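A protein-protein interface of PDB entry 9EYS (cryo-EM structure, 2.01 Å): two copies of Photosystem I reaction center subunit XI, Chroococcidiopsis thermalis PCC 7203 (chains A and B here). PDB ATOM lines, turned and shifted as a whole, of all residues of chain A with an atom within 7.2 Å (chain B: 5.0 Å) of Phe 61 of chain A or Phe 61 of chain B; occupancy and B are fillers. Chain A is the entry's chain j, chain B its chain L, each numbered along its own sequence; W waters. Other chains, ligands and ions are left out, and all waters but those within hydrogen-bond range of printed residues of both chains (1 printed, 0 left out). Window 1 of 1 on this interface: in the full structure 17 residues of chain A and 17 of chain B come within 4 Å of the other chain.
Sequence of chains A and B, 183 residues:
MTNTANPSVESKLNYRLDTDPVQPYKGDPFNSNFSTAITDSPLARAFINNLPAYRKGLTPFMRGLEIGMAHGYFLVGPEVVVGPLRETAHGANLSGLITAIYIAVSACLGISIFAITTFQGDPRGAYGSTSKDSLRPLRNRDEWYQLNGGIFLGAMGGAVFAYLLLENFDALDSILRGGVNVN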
ATOM      1  N   LEU A  58       8.925   5.905   6.308  1.00  0.00           N
ATOM      2  CA  LEU A  58       8.893   5.784   4.857  1.00  0.00           C
ATOM      3  C   LEU A  58       8.159   6.962   4.230  1.00  0.00           C
ATOM      4  O   LEU A  58       7.110   7.393   4.715  1.00  0.00           O
ATOM      5  CB  LEU A  58       8.214   4.477   4.452  1.00  0.00           C
ATOM      6  CG  LEU A  58       9.102   3.264   4.174  1.00  0.00           C
ATOM      7  CD1 LEU A  58       8.269   2.109   3.644  1.00  0.00           C
ATOM      8  CD2 LEU A  58      10.195   3.623   3.193  1.00  0.00           C
ATOM      9  N   THR A  59       8.719   7.485   3.144  1.00  0.00           N
ATOM     10  CA  THR A  59       8.007   8.470   2.353  1.00  0.00           C
ATOM     11  C   THR A  59       6.861   7.793   1.603  1.00  0.00           C
ATOM     12  O   THR A  59       6.941   6.604   1.283  1.00  0.00           O
ATOM     13  CB  THR A  59       8.945   9.156   1.362  1.00  0.00           C
ATOM     14  OG1 THR A  59       9.552   8.174   0.514  1.00  0.00           O
ATOM     15  CG2 THR A  59      10.023   9.928   2.099  1.00  0.00           C
ATOM     16  N   PRO A  60       5.777   8.522   1.324  1.00  0.00           N
ATOM     17  CA  PRO A  60       4.640   7.893   0.632  1.00  0.00           C
ATOM     18  C   PRO A  60       5.010   7.284  -0.708  1.00  0.00           C
ATOM     19  O   PRO A  60       4.474   6.231  -1.072  1.00  0.00           O
ATOM     20  CB  PRO A  60       3.646   9.052   0.478  1.00  0.00           C
ATOM     21  CG  PRO A  60       4.003   9.999   1.565  1.00  0.00           C
ATOM     22  CD  PRO A  60       5.491   9.916   1.703  1.00  0.00           C
ATOM     23  N   PHE A  61       5.919   7.916  -1.453  1.00  0.00           N
ATOM     24  CA  PHE A  61       6.345   7.347  -2.727  1.00  0.00           C
ATOM     25  C   PHE A  61       7.066   6.022  -2.527  1.00  0.00           C
ATOM     26  O   PHE A  61       6.867   5.077  -3.298  1.00  0.00           O
ATOM     27  CB  PHE A  61       7.238   8.335  -3.477  1.00  0.00           C
ATOM     28  CG  PHE A  61       7.689   7.838  -4.818  1.00  0.00           C
ATOM     29  CD1 PHE A  61       6.896   8.020  -5.937  1.00  0.00           C
ATOM     30  CD2 PHE A  61       8.899   7.181  -4.960  1.00  0.00           C
ATOM     31  CE1 PHE A  61       7.303   7.562  -7.172  1.00  0.00           C
ATOM     32  CE2 PHE A  61       9.310   6.720  -6.194  1.00  0.00           C
ATOM     33  CZ  PHE A  61       8.511   6.911  -7.301  1.00  0.00           C
ATOM     34  N   MET A  62       7.920   5.936  -1.504  1.00  0.00           N
ATOM     35  CA  MET A  62       8.630   4.690  -1.242  1.00  0.00           C
ATOM     36  C   MET A  62       7.683   3.586  -0.793  1.00  0.00           C
ATOM     37  O   MET A  62       7.903   2.416  -1.120  1.00  0.00           O
ATOM     38  CB  MET A  62       9.723   4.916  -0.200  1.00  0.00           C
ATOM     39  CG  MET A  62      10.943   4.035  -0.395  1.00  0.00           C
ATOM     40  SD  MET A  62      11.674   4.225  -2.030  1.00  0.00           S
ATOM     41  CE  MET A  62      12.603   2.701  -2.162  1.00  0.00           C
ATOM     42  N   ARG A  63       6.638   3.933  -0.038  1.00  0.00           N
ATOM     43  CA  ARG A  63       5.616   2.950   0.306  1.00  0.00           C
ATOM     44  C   ARG A  63       4.970   2.382  -0.950  1.00  0.00           C
ATOM     45  O   ARG A  63       4.875   1.163  -1.119  1.00  0.00           O
ATOM     46  CB  ARG A  63       4.551   3.579   1.202  1.00  0.00           C
ATOM     47  CG  ARG A  63       5.075   4.280   2.434  1.00  0.00           C
ATOM     48  CD  ARG A  63       3.919   4.729   3.308  1.00  0.00           C
ATOM     49  NE  ARG A  63       4.371   5.461   4.484  1.00  0.00           N
ATOM     50  CZ  ARG A  63       4.763   4.888   5.613  1.00  0.00           C
ATOM     51  NH1 ARG A  63       4.758   3.574   5.757  1.00  0.00           N
ATOM     52  NH2 ARG A  63       5.165   5.654   6.623  1.00  0.00           N
ATOM     53  N   GLY A  64       4.527   3.263  -1.850  1.00  0.00           N
ATOM     54  CA  GLY A  64       3.893   2.807  -3.072  1.00  0.00           C
ATOM     55  C   GLY A  64       4.820   2.011  -3.965  1.00  0.00           C
ATOM     56  O   GLY A  64       4.383   1.079  -4.642  1.00  0.00           O
ATOM     57  N   LEU A  65       6.106   2.366  -3.986  1.00  0.00           N
ATOM     58  CA  LEU A  65       7.052   1.655  -4.838  1.00  0.00           C
ATOM     59  C   LEU A  65       7.181   0.195  -4.423  1.00  0.00           C
ATOM     60  O   LEU A  65       7.135  -0.701  -5.272  1.00  0.00           O
ATOM     61  CB  LEU A  65       8.414   2.345  -4.802  1.00  0.00           C
ATOM     62  CG  LEU A  65       9.470   1.800  -5.764  1.00  0.00           C
ATOM     63  CD1 LEU A  65       9.025   1.978  -7.206  1.00  0.00           C
ATOM     64  CD2 LEU A  65      10.811   2.472  -5.526  1.00  0.00           C
ATOM     65  N   GLU A  66       7.322  -0.068  -3.123  1.00  0.00           N
ATOM     66  CA  GLU A  66       7.476  -1.446  -2.667  1.00  0.00           C
ATOM     67  C   GLU A  66       6.182  -2.233  -2.832  1.00  0.00           C
ATOM     68  O   GLU A  66       6.211  -3.413  -3.198  1.00  0.00           O
ATOM     69  CB  GLU A  66       7.940  -1.476  -1.212  1.00  0.00           C
ATOM     70  CG  GLU A  66       8.273  -2.872  -0.704  1.00  0.00           C
ATOM     71  CD  GLU A  66       8.848  -2.866   0.697  1.00  0.00           C
ATOM     72  OE1 GLU A  66       9.100  -1.768   1.230  1.00  0.00           O
ATOM     73  OE2 GLU A  66       9.053  -3.961   1.264  1.00  0.00           O
ATOM     74  N   ILE A  67       5.038  -1.601  -2.559  1.00  0.00           N
ATOM     75  CA  ILE A  67       3.756  -2.282  -2.728  1.00  0.00           C
ATOM     76  C   ILE A  67       3.524  -2.613  -4.196  1.00  0.00           C
ATOM     77  O   ILE A  67       3.094  -3.719  -4.543  1.00  0.00           O
ATOM     78  CB  ILE A  67       2.613  -1.425  -2.155  1.00  0.00           C
ATOM     79  CG1 ILE A  67       2.803  -1.219  -0.653  1.00  0.00           C
ATOM     80  CG2 ILE A  67       1.271  -2.076  -2.431  1.00  0.00           C
ATOM     81  CD1 ILE A  67       1.902  -0.162  -0.066  1.00  0.00           C
ATOM     82  N   ASP A 142      -1.417  15.107  -0.466  1.00  0.00           N
ATOM     83  CA  ASP A 142      -0.105  14.974  -1.093  1.00  0.00           C
ATOM     84  C   ASP A 142       0.463  13.575  -0.895  1.00  0.00           C
ATOM     85  O   ASP A 142       1.095  13.021  -1.802  1.00  0.00           O
ATOM     86  CB  ASP A 142       0.854  16.022  -0.532  1.00  0.00           C
ATOM     87  CG  ASP A 142       0.545  17.419  -1.028  1.00  0.00           C
ATOM     88  OD1 ASP A 142      -0.252  17.551  -1.979  1.00  0.00           O
ATOM     89  OD2 ASP A 142       1.103  18.386  -0.468  1.00  0.00           O
ATOM     90  N   GLU A 143       0.258  12.991   0.287  1.00  0.00           N
ATOM     91  CA  GLU A 143       0.758  11.646   0.541  1.00  0.00           C
ATOM     92  C   GLU A 143       0.097  10.621  -0.369  1.00  0.00           C
ATOM     93  O   GLU A 143       0.749   9.662  -0.797  1.00  0.00           O
ATOM     94  CB  GLU A 143       0.539  11.270   2.005  1.00  0.00           C
ATOM     95  CG  GLU A 143       1.081  12.287   2.992  1.00  0.00           C
ATOM     96  CD  GLU A 143       1.201  11.730   4.394  1.00  0.00           C
ATOM     97  OE1 GLU A 143       2.287  11.219   4.741  1.00  0.00           O
ATOM     98  OE2 GLU A 143       0.212  11.802   5.152  1.00  0.00           O
ATOM     99  N   TYR A 145      -1.099  11.120  -3.466  1.00  0.00           N
ATOM    100  CA  TYR A 145      -0.591  11.243  -4.827  1.00  0.00           C
ATOM    101  C   TYR A 145       0.840  10.738  -4.943  1.00  0.00           C
ATOM    102  O   TYR A 145       1.209  10.158  -5.969  1.00  0.00           O
ATOM    103  CB  TYR A 145      -0.689  12.690  -5.298  1.00  0.00           C
ATOM    104  CG  TYR A 145      -2.090  13.097  -5.680  1.00  0.00           C
ATOM    105  CD1 TYR A 145      -2.839  12.331  -6.560  1.00  0.00           C
ATOM    106  CD2 TYR A 145      -2.665  14.244  -5.158  1.00  0.00           C
ATOM    107  CE1 TYR A 145      -4.122  12.697  -6.910  1.00  0.00           C
ATOM    108  CE2 TYR A 145      -3.945  14.617  -5.502  1.00  0.00           C
ATOM    109  CZ  TYR A 145      -4.668  13.843  -6.378  1.00  0.00           C
ATOM    110  OH  TYR A 145      -5.943  14.221  -6.720  1.00  0.00           O
ATOM    111  N   GLN A 146       1.660  10.956  -3.914  1.00  0.00           N
ATOM    112  CA  GLN A 146       2.994  10.366  -3.903  1.00  0.00           C
ATOM    113  C   GLN A 146       2.916   8.848  -3.813  1.00  0.00           C
ATOM    114  O   GLN A 146       3.695   8.141  -4.463  1.00  0.00           O
ATOM    115  CB  GLN A 146       3.814  10.937  -2.748  1.00  0.00           C
ATOM    116  CG  GLN A 146       4.380  12.318  -3.020  1.00  0.00           C
ATOM    117  CD  GLN A 146       5.152  12.382  -4.323  1.00  0.00           C
ATOM    118  OE1 GLN A 146       4.631  12.822  -5.347  1.00  0.00           O
ATOM    119  NE2 GLN A 146       6.404  11.940  -4.292  1.00  0.00           N
ATOM    120  N   LEU A 147       1.985   8.332  -3.009  1.00  0.00           N
ATOM    121  CA  LEU A 147       1.786   6.890  -2.936  1.00  0.00           C
ATOM    122  C   LEU A 147       1.344   6.329  -4.280  1.00  0.00           C
ATOM    123  O   LEU A 147       1.837   5.285  -4.717  1.00  0.00           O
ATOM    124  CB  LEU A 147       0.758   6.554  -1.857  1.00  0.00           C
ATOM    125  CG  LEU A 147       0.281   5.101  -1.815  1.00  0.00           C
ATOM    126  CD1 LEU A 147       1.240   4.245  -1.007  1.00  0.00           C
ATOM    127  CD2 LEU A 147      -1.130   5.002  -1.262  1.00  0.00           C
ATOM    128  N   ASN A 148       0.419   7.017  -4.952  1.00  0.00           N
ATOM    129  CA  ASN A 148      -0.100   6.525  -6.224  1.00  0.00           C
ATOM    130  C   ASN A 148       0.986   6.484  -7.291  1.00  0.00           C
ATOM    131  O   ASN A 148       1.044   5.539  -8.087  1.00  0.00           O
ATOM    132  CB  ASN A 148      -1.269   7.393  -6.683  1.00  0.00           C
ATOM    133  CG  ASN A 148      -2.119   6.712  -7.729  1.00  0.00           C
ATOM    134  OD1 ASN A 148      -2.156   5.486  -7.812  1.00  0.00           O
ATOM    135  ND2 ASN A 148      -2.806   7.503  -8.535  1.00  0.00           N
ATOM    136  N   GLY A 149       1.846   7.502  -7.335  1.00  0.00           N
ATOM    137  CA  GLY A 149       2.951   7.480  -8.278  1.00  0.00           C
ATOM    138  C   GLY A 149       3.890   6.315  -8.039  1.00  0.00           C
ATOM    139  O   GLY A 149       4.359   5.678  -8.985  1.00  0.00           O
ATOM    140  N   GLY A 150       4.177   6.021  -6.771  1.00  0.00           N
ATOM    141  CA  GLY A 150       4.984   4.854  -6.460  1.00  0.00           C
ATOM    142  C   GLY A 150       4.282   3.553  -6.798  1.00  0.00           C
ATOM    143  O   GLY A 150       4.917   2.595  -7.244  1.00  0.00           O
ATOM    144  N   ILE A 151       2.966   3.497  -6.577  1.00  0.00           N
ATOM    145  CA  ILE A 151       2.209   2.280  -6.861  1.00  0.00           C
ATOM    146  C   ILE A 151       2.260   1.958  -8.348  1.00  0.00           C
ATOM    147  O   ILE A 151       2.499   0.812  -8.743  1.00  0.00           O
ATOM    148  CB  ILE A 151       0.758   2.419  -6.366  1.00  0.00           C
ATOM    149  CG1 ILE A 151       0.704   2.394  -4.840  1.00  0.00           C
ATOM    150  CG2 ILE A 151      -0.113   1.317  -6.948  1.00  0.00           C
ATOM    151  CD1 ILE A 151       0.848   1.024  -4.251  1.00  0.00           C
ATOM    152  N   LEU A 153       4.435   3.049 -10.769  1.00  0.00           N
ATOM    153  CA  LEU A 153       5.774   2.738 -11.251  1.00  0.00           C
ATOM    154  C   LEU A 153       6.256   1.393 -10.725  1.00  0.00           C
ATOM    155  O   LEU A 153       6.883   0.622 -11.458  1.00  0.00           O
ATOM    156  CB  LEU A 153       6.740   3.854 -10.858  1.00  0.00           C
ATOM    157  CG  LEU A 153       6.561   5.138 -11.666  1.00  0.00           C
ATOM    158  CD1 LEU A 153       7.429   6.250 -11.114  1.00  0.00           C
ATOM    159  CD2 LEU A 153       6.871   4.888 -13.131  1.00  0.00           C
ATOM    160  N   GLY A 154       5.976   1.096  -9.456  1.00  0.00           N
ATOM    161  CA  GLY A 154       6.349  -0.199  -8.913  1.00  0.00           C
ATOM    162  C   GLY A 154       5.599  -1.346  -9.562  1.00  0.00           C
ATOM    163  O   GLY A 154       6.185  -2.386  -9.869  1.00  0.00           O
ATOM    164  N   THR B  59      16.135  18.057  -6.185  1.00  0.00           N
ATOM    165  CA  THR B  59      15.390  17.243  -5.244  1.00  0.00           C
ATOM    166  C   THR B  59      16.073  15.885  -5.097  1.00  0.00           C
ATOM    167  O   THR B  59      16.708  15.400  -6.035  1.00  0.00           O
ATOM    168  CB  THR B  59      13.947  17.056  -5.710  1.00  0.00           C
ATOM    169  OG1 THR B  59      13.934  16.506  -7.032  1.00  0.00           O
ATOM    170  CG2 THR B  59      13.210  18.386  -5.707  1.00  0.00           C
ATOM    171  N   PRO B  60      15.968  15.255  -3.922  1.00  0.00           N
ATOM    172  CA  PRO B  60      16.659  13.967  -3.729  1.00  0.00           C
ATOM    173  C   PRO B  60      16.236  12.906  -4.728  1.00  0.00           C
ATOM    174  O   PRO B  60      17.066  12.089  -5.154  1.00  0.00           O
ATOM    175  CB  PRO B  60      16.281  13.582  -2.291  1.00  0.00           C
ATOM    176  CG  PRO B  60      15.909  14.863  -1.637  1.00  0.00           C
ATOM    177  CD  PRO B  60      15.272  15.697  -2.702  1.00  0.00           C
ATOM    178  N   PHE B  61      14.962  12.905  -5.125  1.00  0.00           N
ATOM    179  CA  PHE B  61      14.499  11.928  -6.102  1.00  0.00           C
ATOM    180  C   PHE B  61      15.202  12.110  -7.440  1.00  0.00           C
ATOM    181  O   PHE B  61      15.556  11.127  -8.095  1.00  0.00           O
ATOM    182  CB  PHE B  61      12.984  12.026  -6.276  1.00  0.00           C
ATOM    183  CG  PHE B  61      12.425  11.016  -7.235  1.00  0.00           C
ATOM    184  CD1 PHE B  61      12.126   9.734  -6.810  1.00  0.00           C
ATOM    185  CD2 PHE B  61      12.212  11.344  -8.563  1.00  0.00           C
ATOM    186  CE1 PHE B  61      11.619   8.799  -7.690  1.00  0.00           C
ATOM    187  CE2 PHE B  61      11.708  10.413  -9.446  1.00  0.00           C
ATOM    188  CZ  PHE B  61      11.409   9.139  -9.009  1.00  0.00           C
ATOM    189  N   MET B  62      15.409  13.357  -7.867  1.00  0.00           N
ATOM    190  CA  MET B  62      16.078  13.594  -9.144  1.00  0.00           C
ATOM    191  C   MET B  62      17.550  13.199  -9.082  1.00  0.00           C
ATOM    192  O   MET B  62      18.093  12.645 -10.050  1.00  0.00           O
ATOM    193  CB  MET B  62      15.925  15.057  -9.552  1.00  0.00           C
ATOM    194  CG  MET B  62      15.888  15.272 -11.053  1.00  0.00           C
ATOM    195  SD  MET B  62      14.504  14.416 -11.825  1.00  0.00           S
ATOM    196  CE  MET B  62      14.967  14.511 -13.550  1.00  0.00           C
ATOM    197  N   ARG B  63      18.214  13.487  -7.958  1.00  0.00           N
ATOM    198  CA  ARG B  63      19.576  13.004  -7.754  1.00  0.00           C
ATOM    199  C   ARG B  63      19.637  11.493  -7.900  1.00  0.00           C
ATOM    200  O   ARG B  63      20.468  10.954  -8.647  1.00  0.00           O
ATOM    201  CB  ARG B  63      20.082  13.407  -6.368  1.00  0.00           C
ATOM    202  CG  ARG B  63      19.829  14.842  -5.956  1.00  0.00           C
ATOM    203  CD  ARG B  63      20.448  15.102  -4.592  1.00  0.00           C
ATOM    204  NE  ARG B  63      20.229  16.466  -4.127  1.00  0.00           N
ATOM    205  CZ  ARG B  63      20.987  17.499  -4.465  1.00  0.00           C
ATOM    206  NH1 ARG B  63      22.027  17.357  -5.269  1.00  0.00           N
ATOM    207  NH2 ARG B  63      20.695  18.703  -3.984  1.00  0.00           N
ATOM    208  N   GLY B  64      18.758  10.792  -7.178  1.00  0.00           N
ATOM    209  CA  GLY B  64      18.726   9.345  -7.275  1.00  0.00           C
ATOM    210  C   GLY B  64      18.437   8.868  -8.680  1.00  0.00           C
ATOM    211  O   GLY B  64      19.021   7.888  -9.142  1.00  0.00           O
ATOM    212  N   LEU B  65      17.542   9.560  -9.384  1.00  0.00           N
ATOM    213  CA  LEU B  65      17.193   9.166 -10.743  1.00  0.00           C
ATOM    214  C   LEU B  65      18.405   9.238 -11.660  1.00  0.00           C
ATOM    215  O   LEU B  65      18.701   8.285 -12.385  1.00  0.00           O
ATOM    216  CB  LEU B  65      16.063  10.050 -11.271  1.00  0.00           C
ATOM    217  CG  LEU B  65      15.477   9.669 -12.632  1.00  0.00           C
ATOM    218  CD1 LEU B  65      14.808   8.306 -12.569  1.00  0.00           C
ATOM    219  CD2 LEU B  65      14.501  10.730 -13.110  1.00  0.00           C
ATOM    220  N   GLN B 146      13.502   9.376  -0.658  1.00  0.00           N
ATOM    221  CA  GLN B 146      13.298   9.862  -2.019  1.00  0.00           C
ATOM    222  C   GLN B 146      14.502   9.545  -2.898  1.00  0.00           C
ATOM    223  O   GLN B 146      14.350   9.146  -4.062  1.00  0.00           O
ATOM    224  CB  GLN B 146      13.017  11.363  -2.006  1.00  0.00           C
ATOM    225  CG  GLN B 146      11.634  11.725  -1.491  1.00  0.00           C
ATOM    226  CD  GLN B 146      10.526  11.052  -2.276  1.00  0.00           C
ATOM    227  OE1 GLN B 146       9.921  10.085  -1.815  1.00  0.00           O
ATOM    228  NE2 GLN B 146      10.251  11.565  -3.470  1.00  0.00           N
ATOM    229  N   LEU B 147      15.709   9.709  -2.349  1.00  0.00           N
ATOM    230  CA  LEU B 147      16.918   9.336  -3.071  1.00  0.00           C
ATOM    231  C   LEU B 147      16.900   7.862  -3.439  1.00  0.00           C
ATOM    232  O   LEU B 147      17.270   7.494  -4.554  1.00  0.00           O
ATOM    233  CB  LEU B 147      18.153   9.642  -2.228  1.00  0.00           C
ATOM    234  CG  LEU B 147      19.485   9.270  -2.885  1.00  0.00           C
ATOM    235  CD1 LEU B 147      19.835  10.250  -3.993  1.00  0.00           C
ATOM    236  CD2 LEU B 147      20.607   9.158  -1.869  1.00  0.00           C
ATOM    237  N   GLY B 149      14.278   5.827  -3.818  1.00  0.00           N
ATOM    238  CA  GLY B 149      13.309   5.588  -4.876  1.00  0.00           C
ATOM    239  C   GLY B 149      13.832   6.005  -6.237  1.00  0.00           C
ATOM    240  O   GLY B 149      13.717   5.260  -7.219  1.00  0.00           O
ATOM    241  N   GLY B 150      14.433   7.195  -6.306  1.00  0.00           N
ATOM    242  CA  GLY B 150      15.047   7.627  -7.550  1.00  0.00           C
ATOM    243  C   GLY B 150      16.159   6.701  -8.001  1.00  0.00           C
ATOM    244  O   GLY B 150      16.275   6.391  -9.187  1.00  0.00           O
ATOM    245  N   LEU B 153      14.575   3.394  -9.415  1.00  0.00           N
ATOM    246  CA  LEU B 153      13.913   3.572 -10.703  1.00  0.00           C
ATOM    247  C   LEU B 153      14.919   3.888 -11.802  1.00  0.00           C
ATOM    248  O   LEU B 153      14.849   3.320 -12.899  1.00  0.00           O
ATOM    249  CB  LEU B 153      12.849   4.661 -10.593  1.00  0.00           C
ATOM    250  CG  LEU B 153      11.630   4.194  -9.796  1.00  0.00           C
ATOM    251  CD1 LEU B 153      10.619   5.306  -9.635  1.00  0.00           C
ATOM    252  CD2 LEU B 153      10.998   2.979 -10.457  1.00  0.00           C
HETATM  253  O   HOH W   1       7.048  10.706  -1.155  1.00  0.00           O
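The backbone NH (N) of Gly 149 of chain B lies within hydrogen-bond range of the side-chain sulfur (SD) of Met 62 of chain A, 3.5 Å away.
OE1 of Gln 146 of chain B sits at hydrogen-bond distance from OG1 of Thr 59 of chain A (3.0 Å).
The backbone NH (N) of Met 62 of chain A sits close to the side-chain hydroxyl (OG1) of Thr 59 of chain A (3.4 Å).
O of Gly 150 of chain A lies close to N of Leu 65 of chain A, 3.5 Å away.
Among the printed residues, merely in contact across the chains: Phe 61 of chain A with Phe 61 of chain B, Phe 61 of chain A with Gln 146 of chain B, Phe 61 of chain A with Leu 153 of chain B, Leu 65 of chain A with Leu 153 of chain B, Gln 146 of chain A with Gln 146 of chain B and Leu 153 of chain A with Leu 153 of chain B.
Phe 61 of chain A touches just these residues of chain B: Phe 61 (3.4 Å), Gln 146 (3.6 Å) and Leu 153 (3.5 Å).
Phe 61 of chain B touches just one residue of chain A: Phe 61 (3.4 Å).
Of the printed residues of chain B, Met 62 of chain A touches Gly 149.
Of the printed residues of chain A, Leu 153 of chain B touches Phe 61, Leu 65 and Leu 153.
Printed residues of chain B within 4 Å of Thr 59 of chain A: Gln 146 (3.0 Å).
Of the printed residues of chain A, Gly 149 of chain B touches Met 62.
Leu 147 of chain A touches none of the printed residues of chain B.
The nearest residue of chain B that does not touch Phe 61 of chain A is Gly 149 of chain B (4.4 Å).
The nearest printed residue of chain A that does not touch Leu 153 of chain B is Gly 154 of chain A (5.5 Å).
Hydrophobic or aromatic side chains of chain A that line the printed part of chain B: Phe 61, Met 62, Leu 65 and Leu 153.
Printed residues of chain B that touch a printed residue of chain A: Phe 61, Gln 146, Gly 149 and Leu 153.
Among the printed residues, 8 pairs touch across the chains.
Among the printed residues, no Asp or Glu carboxylate lies within 4 Å of a Lys or Arg side-chain nitrogen of the other chain.
Phe 61 of chain A touches its own counterpart, Phe 61 of chain B.
Leu 65 of chain A touches Leu 153 of chain B, but with the chains exchanged Leu 153 of chain A does not touch Leu 65 of chain B (7.8 Å).
Gln 146 of chain A touches its own counterpart, Gln 146 of chain B.
Leu 153 of chain B touches its own counterpart, Leu 153 of chain A.
Of the 8 pairs that touch across the chains among the printed residues, 3 have their exchanged pair printed and touching as well.
Water W1 lies within hydrogen-bond range of the side-chain amide oxygen of Gln 146 of chain B (3.0 Å), the backbone NH of Phe 61 of chain A (3.0 Å) and the side-chain amide nitrogen of Gln 146 of chain A (3.4 Å).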
